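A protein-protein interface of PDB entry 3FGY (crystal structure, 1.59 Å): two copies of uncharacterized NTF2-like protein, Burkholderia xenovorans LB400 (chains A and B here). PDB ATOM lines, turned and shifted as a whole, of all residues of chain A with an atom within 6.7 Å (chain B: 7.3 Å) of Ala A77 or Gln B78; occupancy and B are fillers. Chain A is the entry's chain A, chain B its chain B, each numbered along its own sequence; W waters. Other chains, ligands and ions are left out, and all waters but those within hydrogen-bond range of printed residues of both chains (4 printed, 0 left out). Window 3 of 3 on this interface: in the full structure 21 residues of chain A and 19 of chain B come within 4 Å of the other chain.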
ATOM      1  N   THR A   4      17.547  10.978   1.135  1.00  0.00           N
ATOM      2  CA  THR A   4      18.339  12.057   1.775  1.00  0.00           C
ATOM      3  C   THR A   4      17.678  13.454   1.763  1.00  0.00           C
ATOM      4  O   THR A   4      18.256  14.435   2.259  1.00  0.00           O
ATOM      5  CB  THR A   4      19.690  12.212   1.060  1.00  0.00           C
ATOM      6  OG1 THR A   4      19.454  12.605  -0.300  1.00  0.00           O
ATOM      7  CG2 THR A   4      20.483  10.913   1.104  1.00  0.00           C
ATOM      8  N   GLN A   5      16.489  13.540   1.176  1.00  0.00           N
ATOM      9  CA  GLN A   5      15.817  14.819   0.942  1.00  0.00           C
ATOM     10  C   GLN A   5      15.641  15.566   2.254  1.00  0.00           C
ATOM     11  O   GLN A   5      15.880  16.779   2.336  1.00  0.00           O
ATOM     12  CB  GLN A   5      14.431  14.589   0.310  1.00  0.00           C
ATOM     13  CG  GLN A   5      14.407  13.656  -0.909  1.00  0.00           C
ATOM     14  CD  GLN A   5      15.205  14.187  -2.062  1.00  0.00           C
ATOM     15  OE1 GLN A   5      16.107  13.515  -2.574  1.00  0.00           O
ATOM     16  NE2 GLN A   5      14.891  15.412  -2.482  1.00  0.00           N
ATOM     17  N   ASN A   7      17.286  15.043   5.153  1.00  0.00           N
ATOM     18  CA  ASN A   7      18.573  15.461   5.735  1.00  0.00           C
ATOM     19  C   ASN A   7      19.126  16.720   5.089  1.00  0.00           C
ATOM     20  O   ASN A   7      19.655  17.597   5.774  1.00  0.00           O
ATOM     21  CB  ASN A   7      19.620  14.350   5.639  1.00  0.00           C
ATOM     22  CG  ASN A   7      19.319  13.210   6.556  1.00  0.00           C
ATOM     23  OD1 ASN A   7      18.414  13.312   7.379  1.00  0.00           O
ATOM     24  ND2 ASN A   7      20.069  12.116   6.436  1.00  0.00           N
ATOM     25  N   VAL A   8      18.991  16.818   3.769  1.00  0.00           N
ATOM     26  CA  VAL A   8      19.473  18.004   3.059  1.00  0.00           C
ATOM     27  C   VAL A   8      18.667  19.243   3.502  1.00  0.00           C
ATOM     28  O   VAL A   8      19.242  20.319   3.699  1.00  0.00           O
ATOM     29  CB  VAL A   8      19.422  17.833   1.528  1.00  0.00           C
ATOM     30  CG1 VAL A   8      19.617  19.178   0.833  1.00  0.00           C
ATOM     31  CG2 VAL A   8      20.456  16.817   1.068  1.00  0.00           C
ATOM     32  N   PHE A  75      25.233  20.466  -2.424  1.00  0.00           N
ATOM     33  CA  PHE A  75      24.950  19.441  -1.418  1.00  0.00           C
ATOM     34  C   PHE A  75      25.106  18.073  -2.069  1.00  0.00           C
ATOM     35  O   PHE A  75      24.470  17.800  -3.104  1.00  0.00           O
ATOM     36  CB  PHE A  75      23.540  19.613  -0.839  1.00  0.00           C
ATOM     37  CG  PHE A  75      23.361  20.886  -0.110  1.00  0.00           C
ATOM     38  CD1 PHE A  75      23.088  22.059  -0.805  1.00  0.00           C
ATOM     39  CD2 PHE A  75      23.531  20.953   1.259  1.00  0.00           C
ATOM     40  CE1 PHE A  75      22.959  23.253  -0.152  1.00  0.00           C
ATOM     41  CE2 PHE A  75      23.401  22.154   1.910  1.00  0.00           C
ATOM     42  CZ  PHE A  75      23.120  23.299   1.214  1.00  0.00           C
ATOM     43  N   VAL A  76      25.934  17.230  -1.464  1.00  0.00           N
ATOM     44  CA  VAL A  76      26.101  15.855  -1.884  1.00  0.00           C
ATOM     45  C   VAL A  76      25.753  14.981  -0.685  1.00  0.00           C
ATOM     46  O   VAL A  76      26.454  15.040   0.331  1.00  0.00           O
ATOM     47  CB  VAL A  76      27.526  15.566  -2.351  1.00  0.00           C
ATOM     48  CG1 VAL A  76      27.626  14.107  -2.852  1.00  0.00           C
ATOM     49  CG2 VAL A  76      27.936  16.566  -3.444  1.00  0.00           C
ATOM     50  N   ALA A  77      24.685  14.188  -0.823  1.00  0.00           N
ATOM     51  CA  ALA A  77      24.058  13.486   0.289  1.00  0.00           C
ATOM     52  C   ALA A  77      23.948  11.981  -0.008  1.00  0.00           C
ATOM     53  O   ALA A  77      23.517  11.576  -1.090  1.00  0.00           O
ATOM     54  CB  ALA A  77      22.640  14.081   0.583  1.00  0.00           C
ATOM     55  N   GLN A  78      24.314  11.169   0.974  1.00  0.00           N
ATOM     56  CA  GLN A  78      24.156   9.727   0.899  1.00  0.00           C
ATOM     57  C   GLN A  78      24.077   9.209   2.332  1.00  0.00           C
ATOM     58  O   GLN A  78      24.837   9.653   3.214  1.00  0.00           O
ATOM     59  CB  GLN A  78      25.322   9.095   0.122  1.00  0.00           C
ATOM     60  CG  GLN A  78      25.091   7.635  -0.209  1.00  0.00           C
ATOM     61  CD  GLN A  78      26.169   7.048  -1.103  1.00  0.00           C
ATOM     62  OE1 GLN A  78      27.316   7.467  -1.076  1.00  0.00           O
ATOM     63  NE2 GLN A  78      25.792   6.022  -1.880  1.00  0.00           N
ATOM     64  N   GLY A  79      23.111   8.337   2.586  1.00  0.00           N
ATOM     65  CA  GLY A  79      22.950   7.781   3.906  1.00  0.00           C
ATOM     66  C   GLY A  79      22.644   8.886   4.900  1.00  0.00           C
ATOM     67  O   GLY A  79      21.776   9.717   4.654  1.00  0.00           O
ATOM     68  N   ARG A  81      24.806  11.157   5.700  1.00  0.00           N
ATOM     69  CA  ARG A  81      25.815  12.171   5.444  1.00  0.00           C
ATOM     70  C   ARG A  81      25.360  13.212   4.428  1.00  0.00           C
ATOM     71  O   ARG A  81      24.703  12.865   3.455  1.00  0.00           O
ATOM     72  CB  ARG A  81      27.095  11.484   4.956  1.00  0.00           C
ATOM     73  CG  ARG A  81      27.615  10.417   5.921  1.00  0.00           C
ATOM     74  CD  ARG A  81      28.441  11.036   7.021  1.00  0.00           C
ATOM     75  NE  ARG A  81      29.841  11.262   6.629  1.00  0.00           N
ATOM     76  CZ  ARG A  81      30.644  12.163   7.204  1.00  0.00           C
ATOM     77  NH1 ARG A  81      30.216  12.967   8.162  1.00  0.00           N
ATOM     78  NH2 ARG A  81      31.889  12.281   6.795  1.00  0.00           N
ATOM     79  N   VAL A  82      25.689  14.475   4.694  1.00  0.00           N
ATOM     80  CA  VAL A  82      25.507  15.570   3.763  1.00  0.00           C
ATOM     81  C   VAL A  82      26.837  16.314   3.733  1.00  0.00           C
ATOM     82  O   VAL A  82      27.300  16.806   4.752  1.00  0.00           O
ATOM     83  CB  VAL A  82      24.368  16.532   4.212  1.00  0.00           C
ATOM     84  CG1 VAL A  82      24.167  17.611   3.200  1.00  0.00           C
ATOM     85  CG2 VAL A  82      23.065  15.764   4.389  1.00  0.00           C
ATOM     86  N   LEU A  83      27.493  16.304   2.580  1.00  0.00           N
ATOM     87  CA  LEU A  83      28.693  17.084   2.401  1.00  0.00           C
ATOM     88  C   LEU A  83      28.320  18.330   1.625  1.00  0.00           C
ATOM     89  O   LEU A  83      27.675  18.259   0.567  1.00  0.00           O
ATOM     90  CB  LEU A  83      29.762  16.258   1.705  1.00  0.00           C
ATOM     91  CG  LEU A  83      30.652  15.492   2.683  1.00  0.00           C
ATOM     92  CD1 LEU A  83      29.891  14.515   3.597  1.00  0.00           C
ATOM     93  CD2 LEU A  83      31.808  14.811   1.905  1.00  0.00           C
ATOM     94  N   MET B   2      25.197   7.008 -15.236  1.00  0.00           N
ATOM     95  CA  MET B   2      24.658   7.844 -14.153  1.00  0.00           C
ATOM     96  C   MET B   2      24.672   7.135 -12.815  1.00  0.00           C
ATOM     97  O   MET B   2      24.433   7.758 -11.797  1.00  0.00           O
ATOM     98  CB  MET B   2      23.219   8.268 -14.454  1.00  0.00           C
ATOM     99  CG  MET B   2      23.064   9.199 -15.629  1.00  0.00           C
ATOM    100  SD  MET B   2      24.060  10.837 -15.398  1.00  0.00           S
ATOM    101  CE  MET B   2      23.679  11.307 -13.553  1.00  0.00           C
ATOM    102  N   SER B   3      24.893   5.825 -12.802  1.00  0.00           N
ATOM    103  CA  SER B   3      24.879   5.061 -11.543  1.00  0.00           C
ATOM    104  C   SER B   3      25.889   5.558 -10.533  1.00  0.00           C
ATOM    105  O   SER B   3      27.089   5.578 -10.824  1.00  0.00           O
ATOM    106  CB  SER B   3      25.199   3.598 -11.788  1.00  0.00           C
ATOM    107  OG  SER B   3      25.395   2.870 -10.586  1.00  0.00           O
ATOM    108  N   THR B   4      25.411   5.873  -9.328  1.00  0.00           N
ATOM    109  CA  THR B   4      26.276   6.285  -8.220  1.00  0.00           C
ATOM    110  C   THR B   4      27.305   5.181  -7.936  1.00  0.00           C
ATOM    111  O   THR B   4      28.502   5.466  -7.836  1.00  0.00           O
ATOM    112  CB  THR B   4      25.463   6.511  -6.961  1.00  0.00           C
ATOM    113  OG1 THR B   4      24.504   7.511  -7.218  1.00  0.00           O
ATOM    114  CG2 THR B   4      26.317   6.975  -5.817  1.00  0.00           C
ATOM    115  N   ASN B   7      29.942   4.866 -10.610  1.00  0.00           N
ATOM    116  CA  ASN B   7      30.900   5.970 -10.569  1.00  0.00           C
ATOM    117  C   ASN B   7      31.870   5.897  -9.390  1.00  0.00           C
ATOM    118  O   ASN B   7      33.057   6.229  -9.539  1.00  0.00           O
ATOM    119  CB  ASN B   7      30.162   7.296 -10.675  1.00  0.00           C
ATOM    120  CG  ASN B   7      29.588   7.493 -12.067  1.00  0.00           C
ATOM    121  OD1 ASN B   7      30.270   7.199 -13.068  1.00  0.00           O
ATOM    122  ND2 ASN B   7      28.368   8.010 -12.154  1.00  0.00           N
ATOM    123  N   VAL B   8      31.388   5.420  -8.256  1.00  0.00           N
ATOM    124  CA  VAL B   8      32.244   5.138  -7.116  1.00  0.00           C
ATOM    125  C   VAL B   8      33.308   4.100  -7.514  1.00  0.00           C
ATOM    126  O   VAL B   8      34.502   4.284  -7.228  1.00  0.00           O
ATOM    127  CB  VAL B   8      31.427   4.650  -5.913  1.00  0.00           C
ATOM    128  CG1 VAL B   8      32.359   4.018  -4.825  1.00  0.00           C
ATOM    129  CG2 VAL B   8      30.598   5.817  -5.308  1.00  0.00           C
ATOM    130  N   VAL B  76      31.009   9.327  -0.212  1.00  0.00           N
ATOM    131  CA  VAL B  76      29.704   9.963  -0.194  1.00  0.00           C
ATOM    132  C   VAL B  76      29.469  10.431  -1.614  1.00  0.00           C
ATOM    133  O   VAL B  76      30.174  11.308  -2.126  1.00  0.00           O
ATOM    134  CB  VAL B  76      29.673  11.136   0.777  1.00  0.00           C
ATOM    135  CG1 VAL B  76      28.310  11.890   0.724  1.00  0.00           C
ATOM    136  CG2 VAL B  76      30.023  10.655   2.200  1.00  0.00           C
ATOM    137  N   ALA B  77      28.512   9.815  -2.268  1.00  0.00           N
ATOM    138  CA  ALA B  77      28.350   9.996  -3.708  1.00  0.00           C
ATOM    139  C   ALA B  77      26.904  10.111  -4.135  1.00  0.00           C
ATOM    140  O   ALA B  77      26.000   9.550  -3.503  1.00  0.00           O
ATOM    141  CB  ALA B  77      29.021   8.850  -4.462  1.00  0.00           C
ATOM    142  N   GLN B  78      26.707  10.835  -5.238  1.00  0.00           N
ATOM    143  CA  GLN B  78      25.402  11.033  -5.823  1.00  0.00           C
ATOM    144  C   GLN B  78      25.641  11.166  -7.327  1.00  0.00           C
ATOM    145  O   GLN B  78      26.192  12.173  -7.779  1.00  0.00           O
ATOM    146  CB  GLN B  78      24.842  12.324  -5.216  1.00  0.00           C
ATOM    147  CG  GLN B  78      23.408  12.447  -4.925  1.00  0.00           C
ATOM    148  CD  GLN B  78      23.118  13.854  -4.362  1.00  0.00           C
ATOM    149  OE1 GLN B  78      23.175  14.062  -3.165  1.00  0.00           O
ATOM    150  NE2 GLN B  78      22.890  14.828  -5.249  1.00  0.00           N
ATOM    151  N   GLY B  79      25.272  10.148  -8.093  1.00  0.00           N
ATOM    152  CA  GLY B  79      25.380  10.173  -9.539  1.00  0.00           C
ATOM    153  C   GLY B  79      26.824  10.255  -9.979  1.00  0.00           C
ATOM    154  O   GLY B  79      27.624   9.407  -9.628  1.00  0.00           O
ATOM    155  N   GLU B  80      27.163  11.301 -10.720  1.00  0.00           N
ATOM    156  CA  GLU B  80      28.519  11.512 -11.222  1.00  0.00           C
ATOM    157  C   GLU B  80      29.441  12.267 -10.276  1.00  0.00           C
ATOM    158  O   GLU B  80      30.612  12.507 -10.592  1.00  0.00           O
ATOM    159  CB  GLU B  80      28.416  12.231 -12.553  1.00  0.00           C
ATOM    160  CG  GLU B  80      27.985  11.291 -13.656  1.00  0.00           C
ATOM    161  CD  GLU B  80      28.074  11.873 -15.063  1.00  0.00           C
ATOM    162  OE1 GLU B  80      27.665  13.030 -15.247  1.00  0.00           O
ATOM    163  OE2 GLU B  80      28.554  11.132 -15.937  1.00  0.00           O
ATOM    164  N   ARG B  81      28.929  12.608  -9.110  1.00  0.00           N
ATOM    165  CA  ARG B  81      29.683  13.306  -8.113  1.00  0.00           C
ATOM    166  C   ARG B  81      30.061  12.343  -6.988  1.00  0.00           C
ATOM    167  O   ARG B  81      29.194  11.771  -6.309  1.00  0.00           O
ATOM    168  CB  ARG B  81      28.809  14.435  -7.633  1.00  0.00           C
ATOM    169  CG  ARG B  81      29.460  15.509  -7.047  1.00  0.00           C
ATOM    170  CD  ARG B  81      30.357  16.318  -8.008  1.00  0.00           C
ATOM    171  NE  ARG B  81      30.747  17.401  -7.141  1.00  0.00           N
ATOM    172  CZ  ARG B  81      31.961  17.915  -7.045  1.00  0.00           C
ATOM    173  NH1 ARG B  81      32.961  17.473  -7.768  1.00  0.00           N
ATOM    174  NH2 ARG B  81      32.162  18.867  -6.165  1.00  0.00           N
ATOM    175  N   VAL B  82      31.364  12.180  -6.785  1.00  0.00           N
ATOM    176  CA  VAL B  82      31.937  11.229  -5.825  1.00  0.00           C
ATOM    177  C   VAL B  82      32.893  11.953  -4.907  1.00  0.00           C
ATOM    178  O   VAL B  82      33.922  12.474  -5.365  1.00  0.00           O
ATOM    179  CB  VAL B  82      32.691  10.076  -6.508  1.00  0.00           C
ATOM    180  CG1 VAL B  82      33.277   9.113  -5.477  1.00  0.00           C
ATOM    181  CG2 VAL B  82      31.747   9.362  -7.488  1.00  0.00           C
ATOM    182  N   LEU B  83      32.532  12.025  -3.634  1.00  0.00           N
ATOM    183  CA  LEU B  83      33.341  12.676  -2.592  1.00  0.00           C
ATOM    184  C   LEU B  83      33.977  11.605  -1.723  1.00  0.00           C
ATOM    185  O   LEU B  83      33.293  10.715  -1.191  1.00  0.00           O
ATOM    186  CB  LEU B  83      32.517  13.675  -1.751  1.00  0.00           C
ATOM    187  CG  LEU B  83      32.393  15.116  -2.281  1.00  0.00           C
ATOM    188  CD1 LEU B  83      32.123  15.180  -3.768  1.00  0.00           C
ATOM    189  CD2 LEU B  83      31.316  15.880  -1.467  1.00  0.00           C
ATOM    190  N   ILE B 107      35.266  14.637  -6.557  1.00  0.00           N
ATOM    191  CA  ILE B 107      35.537  14.141  -7.897  1.00  0.00           C
ATOM    192  C   ILE B 107      34.262  14.209  -8.701  1.00  0.00           C
ATOM    193  O   ILE B 107      33.187  13.844  -8.204  1.00  0.00           O
ATOM    194  CB  ILE B 107      36.087  12.680  -7.874  1.00  0.00           C
ATOM    195  CG1 ILE B 107      37.329  12.662  -6.956  1.00  0.00           C
ATOM    196  CG2 ILE B 107      36.377  12.160  -9.275  1.00  0.00           C
ATOM    197  CD1 ILE B 107      38.004  11.332  -6.773  1.00  0.00           C
HETATM  198  O   HOH W   1      23.826  17.969  -5.582  1.00  0.00           O
HETATM  199  O   HOH W   2      21.705  16.189  -2.369  1.00  0.00           O
HETATM  200  O   HOH W   3      23.456   9.092  -3.178  1.00  0.00           O
HETATM  201  O   HOH W   4      21.247  12.190  -2.497  1.00  0.00           O
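Val A76 touches its own counterpart, Val B76. Val A76 touches Gln B78, and with the chains exchanged Gln A78 touches Val B76. Val A76 touches Leu B83, but with the chains exchanged Leu A83 does not touch Val B76 (4.1 Å). Leu B83 touches its own counterpart, Leu A83. 10 positions are printed for both chains.
Among the printed residues, merely in contact across the chains: Leu A83 with Leu B83 (3.6 Å), Gln A78 with Val B76 (3.6 Å), Val A76 with Gln B78 (3.7 Å), Val A76 with Val B76 (3.7 Å), Val A76 with Leu B83 (3.9 Å) and Phe A75 with Gln B78 (3.96 Å).
Hydrophobic or aromatic side chains of chain B that line the printed part of chain A: Val B76 and Leu B83. Of the 12 printed residues of chain A, 5 touch a printed residue of chain B. Hydrophobic or aromatic side chains of chain A that line the printed part of chain B: Val A76, Ala A77 and Leu A83. Among the printed residues, 8 pairs touch across the chains. Among the printed residues, no Asp or Glu carboxylate lies within 4 Å of a Lys or Arg side-chain nitrogen of the other chain.
Of the printed residues of chain B, Ala A77 touches Gln B78. Gln B78 touches three residues of chain A. Printed residues of chain B within 4 Å of Leu A83: Leu B83. Of the printed residues of chain A, Ala B77 touches Gln A78 (2.9 Å). Of the printed residues of chain B, Gln A78 touches Val B76 (3.6 Å) and Ala B77 (2.9 Å). Printed residues of chain A within 4 Å of Leu B83: Val A76 and Leu A83. Ser B3 touches none of the printed residues of chain A. The nearest residue of chain A that does not touch Gln B78 is Thr A4 (4.9 Å). The nearest printed residue of chain A that does not touch Ala B77 is Ala A77 (4.01 Å).
O of Val A76 lies within hydrogen-bond range of N of Leu A83. O of Leu B83 sits at hydrogen-bond distance from N of Val B76 (2.8 Å).
Water W1 bridges the backbone carbonyl oxygen (O) of Phe A75 and the side-chain amide nitrogen (NE2) of Gln B78. Water W3 bridges O of Ala B77 (2.6 Å) and O of Ala A77 (3.2 Å). Water W2 bridges OE1 of Gln B78 (2.7 Å) and O of Phe A75 (3.3 Å). Water W4 lies within hydrogen-bond range of the backbone carbonyl oxygen (O) of Ala A77 (2.7 Å), the side-chain amide oxygen (OE1) of Gln B78 (2.8 Å) and the side-chain hydroxyl (OG1) of Thr A4 (2.9 Å).
The backbone NH (N) of Ala A77 lies within hydrogen-bond range of the side-chain amide oxygen (OE1) of Gln B78 (2.8 Å). The side-chain amide oxygen of Gln A78 lies within hydrogen-bond range of the backbone NH of Ala B77 (2.9 Å).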
